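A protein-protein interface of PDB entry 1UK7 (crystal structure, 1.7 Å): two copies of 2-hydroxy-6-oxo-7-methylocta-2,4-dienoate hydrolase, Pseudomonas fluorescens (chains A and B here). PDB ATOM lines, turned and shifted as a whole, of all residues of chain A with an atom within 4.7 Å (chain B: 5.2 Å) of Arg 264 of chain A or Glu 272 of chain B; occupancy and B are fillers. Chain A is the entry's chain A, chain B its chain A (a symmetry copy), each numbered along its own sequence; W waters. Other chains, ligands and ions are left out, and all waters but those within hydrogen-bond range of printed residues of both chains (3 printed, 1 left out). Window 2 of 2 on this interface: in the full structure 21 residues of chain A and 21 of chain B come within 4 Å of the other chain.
Glu 268 of chain B touches its own counterpart, Glu 268 of chain A. Of the 6 pairs that touch across the chains among the printed residues, 1 has its exchanged pair printed and touching as well.
Water W3 bridges NH2 of Arg 264 of chain A and O of Glu 268 of chain B. Water W1 lies within hydrogen-bond range of OE2 of Glu 268 of chain A and OE1 of Glu 268 of chain B. Water W2 lies within hydrogen-bond range of OE2 of Glu 215 of chain B (3.0 Å) and NH2 of Arg 261 of chain A (3.3 Å).
Of chain A, only Arg 261 (2.8 Å) and Arg 264 (3.1 Å) come within 4 Å of Glu 272 of chain B. Of the printed residues of chain A, Glu 268 of chain B touches Arg 264 and Glu 268. Printed residues of chain A within 4 Å of Gln 243 of chain B: Arg 261. Of the printed residues of chain A, Glu 215 of chain B touches Arg 261 (2.9 Å). The nearest residue of chain B that does not touch Arg 264 of chain A is Phe 269 of chain B (4.9 Å). The nearest printed residue of chain A that does not touch Glu 272 of chain B is Asp 260 of chain A (5.7 Å). The nearest printed residue of chain A that does not touch Glu 268 of chain B is Leu 265 of chain A (5.5 Å).
Of the 9 printed residues of chain A, 3 touch a printed residue of chain B. Printed residues of chain A that touch a printed residue of chain B: Arg 261, Arg 264 and Glu 268. Among the printed residues, 6 pairs touch across the chains. Among the printed residues, Asp or Glu carboxylates within 4 Å of a Lys or Arg side-chain nitrogen of the other chain: Arg 261 of chain A with Glu 215 of chain B (2.9 Å), Arg 261 of chain A with Glu 272 of chain B (2.8 Å) and Arg 264 of chain A with Glu 272 of chain B (3.1 Å).
The backbone carbonyl oxygen (O) of Asp 260 of chain A is in hydrogen-bond range of the guanidinium group (NE) of Arg 264 of chain A (3.2 Å). NH1 of Arg 122 of chain B is in salt-bridge range of OE2 of Glu 272 of chain B (2.9 Å).
The guanidinium group of Arg 261 of chain A sits close to the side-chain amide nitrogen of Gln 243 of chain B (3.4 Å). The guanidinium group (NH1) of Arg 264 of chain A is in salt-bridge range of the side-chain carboxylate (OE1) of Glu 272 of chain B (3.1 Å). The side-chain carboxylate of Glu 268 of chain A lies close to the side-chain carboxylate of Glu 268 of chain B (2.5 Å). NH2 of Arg 264 of chain A lies within hydrogen-bond range of O of Glu 268 of chain B, at 3.4 Å. The guanidinium group of Arg 261 of chain A lies within salt-bridge range of the side-chain carboxylate of Glu 215 of chain B (2.9 Å). The guanidinium group (NE) of Arg 261 of chain A is in salt-bridge range of the side-chain carboxylate (OE1) of Glu 272 of chain B (2.8 Å).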
ATOM      1  N   ASP A 260     -10.616 -22.786 -18.353  1.00  0.00           N
ATOM      2  CA  ASP A 260      -9.273 -22.815 -17.782  1.00  0.00           C
ATOM      3  C   ASP A 260      -9.224 -22.401 -16.314  1.00  0.00           C
ATOM      4  O   ASP A 260      -8.551 -23.037 -15.508  1.00  0.00           O
ATOM      5  CB  ASP A 260      -8.321 -21.959 -18.620  1.00  0.00           C
ATOM      6  CG  ASP A 260      -8.131 -22.509 -20.024  1.00  0.00           C
ATOM      7  OD1 ASP A 260      -8.201 -23.747 -20.196  1.00  0.00           O
ATOM      8  OD2 ASP A 260      -7.901 -21.708 -20.953  1.00  0.00           O
ATOM      9  N   ARG A 261      -9.945 -21.345 -15.961  1.00  0.00           N
ATOM     10  CA  ARG A 261      -9.977 -20.891 -14.572  1.00  0.00           C
ATOM     11  C   ARG A 261     -10.623 -21.959 -13.690  1.00  0.00           C
ATOM     12  O   ARG A 261     -10.145 -22.248 -12.593  1.00  0.00           O
ATOM     13  CB  ARG A 261     -10.774 -19.591 -14.461  1.00  0.00           C
ATOM     14  CG  ARG A 261     -10.071 -18.379 -15.041  1.00  0.00           C
ATOM     15  CD  ARG A 261     -10.995 -17.177 -15.064  1.00  0.00           C
ATOM     16  NE  ARG A 261     -10.275 -15.950 -15.381  1.00  0.00           N
ATOM     17  CZ  ARG A 261     -10.853 -14.762 -15.504  1.00  0.00           C
ATOM     18  NH1 ARG A 261     -12.163 -14.643 -15.346  1.00  0.00           N
ATOM     19  NH2 ARG A 261     -10.113 -13.688 -15.756  1.00  0.00           N
ATOM     20  N   PHE A 262     -11.718 -22.531 -14.183  1.00  0.00           N
ATOM     21  CA  PHE A 262     -12.458 -23.569 -13.468  1.00  0.00           C
ATOM     22  C   PHE A 262     -11.577 -24.787 -13.204  1.00  0.00           C
ATOM     23  O   PHE A 262     -11.472 -25.258 -12.073  1.00  0.00           O
ATOM     24  CB  PHE A 262     -13.677 -23.996 -14.295  1.00  0.00           C
ATOM     25  CG  PHE A 262     -14.459 -25.127 -13.686  1.00  0.00           C
ATOM     26  CD1 PHE A 262     -15.443 -24.877 -12.738  1.00  0.00           C
ATOM     27  CD2 PHE A 262     -14.202 -26.446 -14.056  1.00  0.00           C
ATOM     28  CE1 PHE A 262     -16.164 -25.919 -12.164  1.00  0.00           C
ATOM     29  CE2 PHE A 262     -14.917 -27.501 -13.487  1.00  0.00           C
ATOM     30  CZ  PHE A 262     -15.900 -27.237 -12.541  1.00  0.00           C
ATOM     31  N   ASN A 263     -10.946 -25.296 -14.255  1.00  0.00           N
ATOM     32  CA  ASN A 263     -10.089 -26.466 -14.118  1.00  0.00           C
ATOM     33  C   ASN A 263      -8.943 -26.245 -13.136  1.00  0.00           C
ATOM     34  O   ASN A 263      -8.629 -27.125 -12.338  1.00  0.00           O
ATOM     35  CB  ASN A 263      -9.544 -26.878 -15.482  1.00  0.00           C
ATOM     36  CG  ASN A 263     -10.629 -27.388 -16.400  1.00  0.00           C
ATOM     37  OD1 ASN A 263     -11.710 -27.757 -15.942  1.00  0.00           O
ATOM     38  ND2 ASN A 263     -10.346 -27.431 -17.702  1.00  0.00           N
ATOM     39  N   ARG A 264      -8.320 -25.072 -13.193  1.00  0.00           N
ATOM     40  CA  ARG A 264      -7.217 -24.758 -12.284  1.00  0.00           C
ATOM     41  C   ARG A 264      -7.702 -24.738 -10.835  1.00  0.00           C
ATOM     42  O   ARG A 264      -7.059 -25.294  -9.946  1.00  0.00           O
ATOM     43  CB  ARG A 264      -6.606 -23.399 -12.636  1.00  0.00           C
ATOM     44  CG  ARG A 264      -5.545 -23.445 -13.726  1.00  0.00           C
ATOM     45  CD  ARG A 264      -5.023 -22.053 -14.026  1.00  0.00           C
ATOM     46  NE  ARG A 264      -5.969 -21.286 -14.831  1.00  0.00           N
ATOM     47  CZ  ARG A 264      -6.008 -19.960 -14.880  1.00  0.00           C
ATOM     48  NH1 ARG A 264      -6.900 -19.347 -15.647  1.00  0.00           N
ATOM     49  NH2 ARG A 264      -5.168 -19.245 -14.146  1.00  0.00           N
ATOM     50  N   LEU A 265      -8.839 -24.090 -10.606  1.00  0.00           N
ATOM     51  CA  LEU A 265      -9.406 -23.999  -9.264  1.00  0.00           C
ATOM     52  C   LEU A 265      -9.716 -25.373  -8.694  1.00  0.00           C
ATOM     53  O   LEU A 265      -9.372 -25.673  -7.552  1.00  0.00           O
ATOM     54  CB  LEU A 265     -10.691 -23.170  -9.281  1.00  0.00           C
ATOM     55  CG  LEU A 265     -10.560 -21.648  -9.258  1.00  0.00           C
ATOM     56  CD1 LEU A 265     -11.922 -21.013  -9.493  1.00  0.00           C
ATOM     57  CD2 LEU A 265      -9.987 -21.206  -7.912  1.00  0.00           C
ATOM     58  N   VAL A 266     -10.372 -26.202  -9.495  1.00  0.00           N
ATOM     59  CA  VAL A 266     -10.743 -27.537  -9.053  1.00  0.00           C
ATOM     60  C   VAL A 266      -9.534 -28.439  -8.793  1.00  0.00           C
ATOM     61  O   VAL A 266      -9.464 -29.094  -7.756  1.00  0.00           O
ATOM     62  CB  VAL A 266     -11.681 -28.211 -10.073  1.00  0.00           C
ATOM     63  CG1 VAL A 266     -11.983 -29.642  -9.646  1.00  0.00           C
ATOM     64  CG2 VAL A 266     -12.972 -27.412 -10.177  1.00  0.00           C
ATOM     65  N   VAL A 267      -8.575 -28.464  -9.714  1.00  0.00           N
ATOM     66  CA  VAL A 267      -7.405 -29.315  -9.521  1.00  0.00           C
ATOM     67  C   VAL A 267      -6.619 -28.933  -8.270  1.00  0.00           C
ATOM     68  O   VAL A 267      -6.214 -29.804  -7.505  1.00  0.00           O
ATOM     69  CB  VAL A 267      -6.457 -29.283 -10.745  1.00  0.00           C
ATOM     70  CG1 VAL A 267      -5.185 -30.078 -10.438  1.00  0.00           C
ATOM     71  CG2 VAL A 267      -7.155 -29.886 -11.954  1.00  0.00           C
ATOM     72  N   GLU A 268      -6.408 -27.638  -8.053  1.00  0.00           N
ATOM     73  CA  GLU A 268      -5.659 -27.200  -6.879  1.00  0.00           C
ATOM     74  C   GLU A 268      -6.441 -27.458  -5.604  1.00  0.00           C
ATOM     75  O   GLU A 268      -5.856 -27.720  -4.553  1.00  0.00           O
ATOM     76  CB  GLU A 268      -5.309 -25.716  -6.984  1.00  0.00           C
ATOM     77  CG  GLU A 268      -4.317 -25.404  -8.088  1.00  0.00           C
ATOM     78  CD  GLU A 268      -3.984 -23.934  -8.169  1.00  0.00           C
ATOM     79  OE1 GLU A 268      -4.925 -23.116  -8.152  1.00  0.00           O
ATOM     80  OE2 GLU A 268      -2.785 -23.596  -8.257  1.00  0.00           O
ATOM     81  N   ARG B 122      -3.915  -5.368 -13.596  1.00  0.00           N
ATOM     82  CA  ARG B 122      -4.886  -6.154 -12.842  1.00  0.00           C
ATOM     83  C   ARG B 122      -4.881  -5.748 -11.374  1.00  0.00           C
ATOM     84  O   ARG B 122      -3.878  -5.242 -10.862  1.00  0.00           O
ATOM     85  CB  ARG B 122      -4.593  -7.649 -12.974  1.00  0.00           C
ATOM     86  CG  ARG B 122      -4.688  -8.144 -14.411  1.00  0.00           C
ATOM     87  CD  ARG B 122      -4.816  -9.657 -14.492  1.00  0.00           C
ATOM     88  NE  ARG B 122      -5.199 -10.065 -15.846  1.00  0.00           N
ATOM     89  CZ  ARG B 122      -5.803 -11.211 -16.148  1.00  0.00           C
ATOM     90  NH1 ARG B 122      -6.100 -12.082 -15.192  1.00  0.00           N
ATOM     91  NH2 ARG B 122      -6.134 -11.477 -17.409  1.00  0.00           N
ATOM     92  N   GLU B 215      -9.176  -6.358 -15.046  1.00  0.00           N
ATOM     93  CA  GLU B 215      -9.509  -7.704 -14.608  1.00  0.00           C
ATOM     94  C   GLU B 215      -9.283  -7.560 -13.109  1.00  0.00           C
ATOM     95  O   GLU B 215      -8.222  -7.089 -12.685  1.00  0.00           O
ATOM     96  CB  GLU B 215      -8.530  -8.733 -15.182  1.00  0.00           C
ATOM     97  CG  GLU B 215      -8.846  -9.225 -16.600  1.00  0.00           C
ATOM     98  CD  GLU B 215     -10.090 -10.104 -16.665  1.00  0.00           C
ATOM     99  OE1 GLU B 215     -10.409 -10.758 -15.648  1.00  0.00           O
ATOM    100  OE2 GLU B 215     -10.740 -10.158 -17.735  1.00  0.00           O
ATOM    101  N   GLN B 243     -13.940 -11.275 -10.288  1.00  0.00           N
ATOM    102  CA  GLN B 243     -14.087 -12.619  -9.756  1.00  0.00           C
ATOM    103  C   GLN B 243     -14.110 -12.382  -8.256  1.00  0.00           C
ATOM    104  O   GLN B 243     -13.428 -11.485  -7.759  1.00  0.00           O
ATOM    105  CB  GLN B 243     -12.883 -13.497 -10.085  1.00  0.00           C
ATOM    106  CG  GLN B 243     -12.754 -13.893 -11.537  1.00  0.00           C
ATOM    107  CD  GLN B 243     -11.563 -14.797 -11.765  1.00  0.00           C
ATOM    108  OE1 GLN B 243     -11.576 -15.976 -11.406  1.00  0.00           O
ATOM    109  NE2 GLN B 243     -10.517 -14.243 -12.356  1.00  0.00           N
ATOM    110  N   VAL B 267      -1.139 -15.535  -7.709  1.00  0.00           N
ATOM    111  CA  VAL B 267      -0.140 -15.802  -8.738  1.00  0.00           C
ATOM    112  C   VAL B 267      -0.774 -16.263 -10.048  1.00  0.00           C
ATOM    113  O   VAL B 267      -0.389 -15.799 -11.117  1.00  0.00           O
ATOM    114  CB  VAL B 267       0.897 -16.857  -8.280  1.00  0.00           C
ATOM    115  CG1 VAL B 267       1.836 -17.202  -9.438  1.00  0.00           C
ATOM    116  CG2 VAL B 267       1.706 -16.312  -7.114  1.00  0.00           C
ATOM    117  N   GLU B 268      -1.749 -17.164  -9.970  1.00  0.00           N
ATOM    118  CA  GLU B 268      -2.398 -17.654 -11.183  1.00  0.00           C
ATOM    119  C   GLU B 268      -3.229 -16.565 -11.836  1.00  0.00           C
ATOM    120  O   GLU B 268      -3.368 -16.532 -13.058  1.00  0.00           O
ATOM    121  CB  GLU B 268      -3.278 -18.865 -10.874  1.00  0.00           C
ATOM    122  CG  GLU B 268      -2.492 -20.092 -10.455  1.00  0.00           C
ATOM    123  CD  GLU B 268      -3.382 -21.276 -10.159  1.00  0.00           C
ATOM    124  OE1 GLU B 268      -4.376 -21.096  -9.430  1.00  0.00           O
ATOM    125  OE2 GLU B 268      -3.083 -22.386 -10.648  1.00  0.00           O
ATOM    126  N   PHE B 269      -3.789 -15.679 -11.019  1.00  0.00           N
ATOM    127  CA  PHE B 269      -4.593 -14.583 -11.537  1.00  0.00           C
ATOM    128  C   PHE B 269      -3.685 -13.679 -12.369  1.00  0.00           C
ATOM    129  O   PHE B 269      -4.024 -13.310 -13.490  1.00  0.00           O
ATOM    130  CB  PHE B 269      -5.226 -13.808 -10.376  1.00  0.00           C
ATOM    131  CG  PHE B 269      -5.957 -12.554 -10.795  1.00  0.00           C
ATOM    132  CD1 PHE B 269      -7.026 -12.609 -11.688  1.00  0.00           C
ATOM    133  CD2 PHE B 269      -5.584 -11.318 -10.275  1.00  0.00           C
ATOM    134  CE1 PHE B 269      -7.715 -11.446 -12.053  1.00  0.00           C
ATOM    135  CE2 PHE B 269      -6.265 -10.153 -10.633  1.00  0.00           C
ATOM    136  CZ  PHE B 269      -7.333 -10.217 -11.523  1.00  0.00           C
ATOM    137  N   PHE B 270      -2.519 -13.339 -11.828  1.00  0.00           N
ATOM    138  CA  PHE B 270      -1.588 -12.486 -12.560  1.00  0.00           C
ATOM    139  C   PHE B 270      -0.957 -13.232 -13.737  1.00  0.00           C
ATOM    140  O   PHE B 270      -0.674 -12.631 -14.774  1.00  0.00           O
ATOM    141  CB  PHE B 270      -0.488 -11.954 -11.631  1.00  0.00           C
ATOM    142  CG  PHE B 270      -0.976 -10.974 -10.594  1.00  0.00           C
ATOM    143  CD1 PHE B 270      -2.097 -10.184 -10.829  1.00  0.00           C
ATOM    144  CD2 PHE B 270      -0.288 -10.816  -9.392  1.00  0.00           C
ATOM    145  CE1 PHE B 270      -2.524  -9.249  -9.889  1.00  0.00           C
ATOM    146  CE2 PHE B 270      -0.707  -9.882  -8.443  1.00  0.00           C
ATOM    147  CZ  PHE B 270      -1.829  -9.098  -8.695  1.00  0.00           C
ATOM    148  N   ASN B 271      -0.733 -14.537 -13.576  1.00  0.00           N
ATOM    149  CA  ASN B 271      -0.142 -15.347 -14.647  1.00  0.00           C
ATOM    150  C   ASN B 271      -0.993 -15.291 -15.912  1.00  0.00           C
ATOM    151  O   ASN B 271      -0.471 -15.377 -17.027  1.00  0.00           O
ATOM    152  CB  ASN B 271       0.007 -16.812 -14.207  1.00  0.00           C
ATOM    153  CG  ASN B 271       1.198 -17.039 -13.282  1.00  0.00           C
ATOM    154  OD1 ASN B 271       1.403 -18.147 -12.781  1.00  0.00           O
ATOM    155  ND2 ASN B 271       1.991 -15.999 -13.060  1.00  0.00           N
ATOM    156  N   GLU B 272      -2.301 -15.140 -15.733  1.00  0.00           N
ATOM    157  CA  GLU B 272      -3.235 -15.077 -16.851  1.00  0.00           C
ATOM    158  C   GLU B 272      -2.913 -13.920 -17.792  1.00  0.00           C
ATOM    159  O   GLU B 272      -3.115 -14.020 -19.005  1.00  0.00           O
ATOM    160  CB  GLU B 272      -4.667 -14.915 -16.335  1.00  0.00           C
ATOM    161  CG  GLU B 272      -5.556 -16.123 -16.523  1.00  0.00           C
ATOM    162  CD  GLU B 272      -7.023 -15.780 -16.356  1.00  0.00           C
ATOM    163  OE1 GLU B 272      -7.878 -16.591 -16.763  1.00  0.00           O
ATOM    164  OE2 GLU B 272      -7.322 -14.694 -15.813  1.00  0.00           O
ATOM    165  N   ALA B 273      -2.423 -12.823 -17.223  1.00  0.00           N
ATOM    166  CA  ALA B 273      -2.080 -11.636 -18.000  1.00  0.00           C
ATOM    167  C   ALA B 273      -0.914 -11.900 -18.949  1.00  0.00           C
ATOM    168  O   ALA B 273      -1.053 -11.596 -20.152  1.00  0.00           O
ATOM    169  CB  ALA B 273      -1.741 -10.480 -17.065  1.00  0.00           C
HETATM  170  O   HOH W   1      -1.282 -21.257  -7.819  1.00  0.00           O
HETATM  171  O   HOH W   2     -10.334 -12.805 -18.977  1.00  0.00           O
HETATM  172  O   HOH W   3      -2.790 -18.890 -14.664  1.00  0.00           O
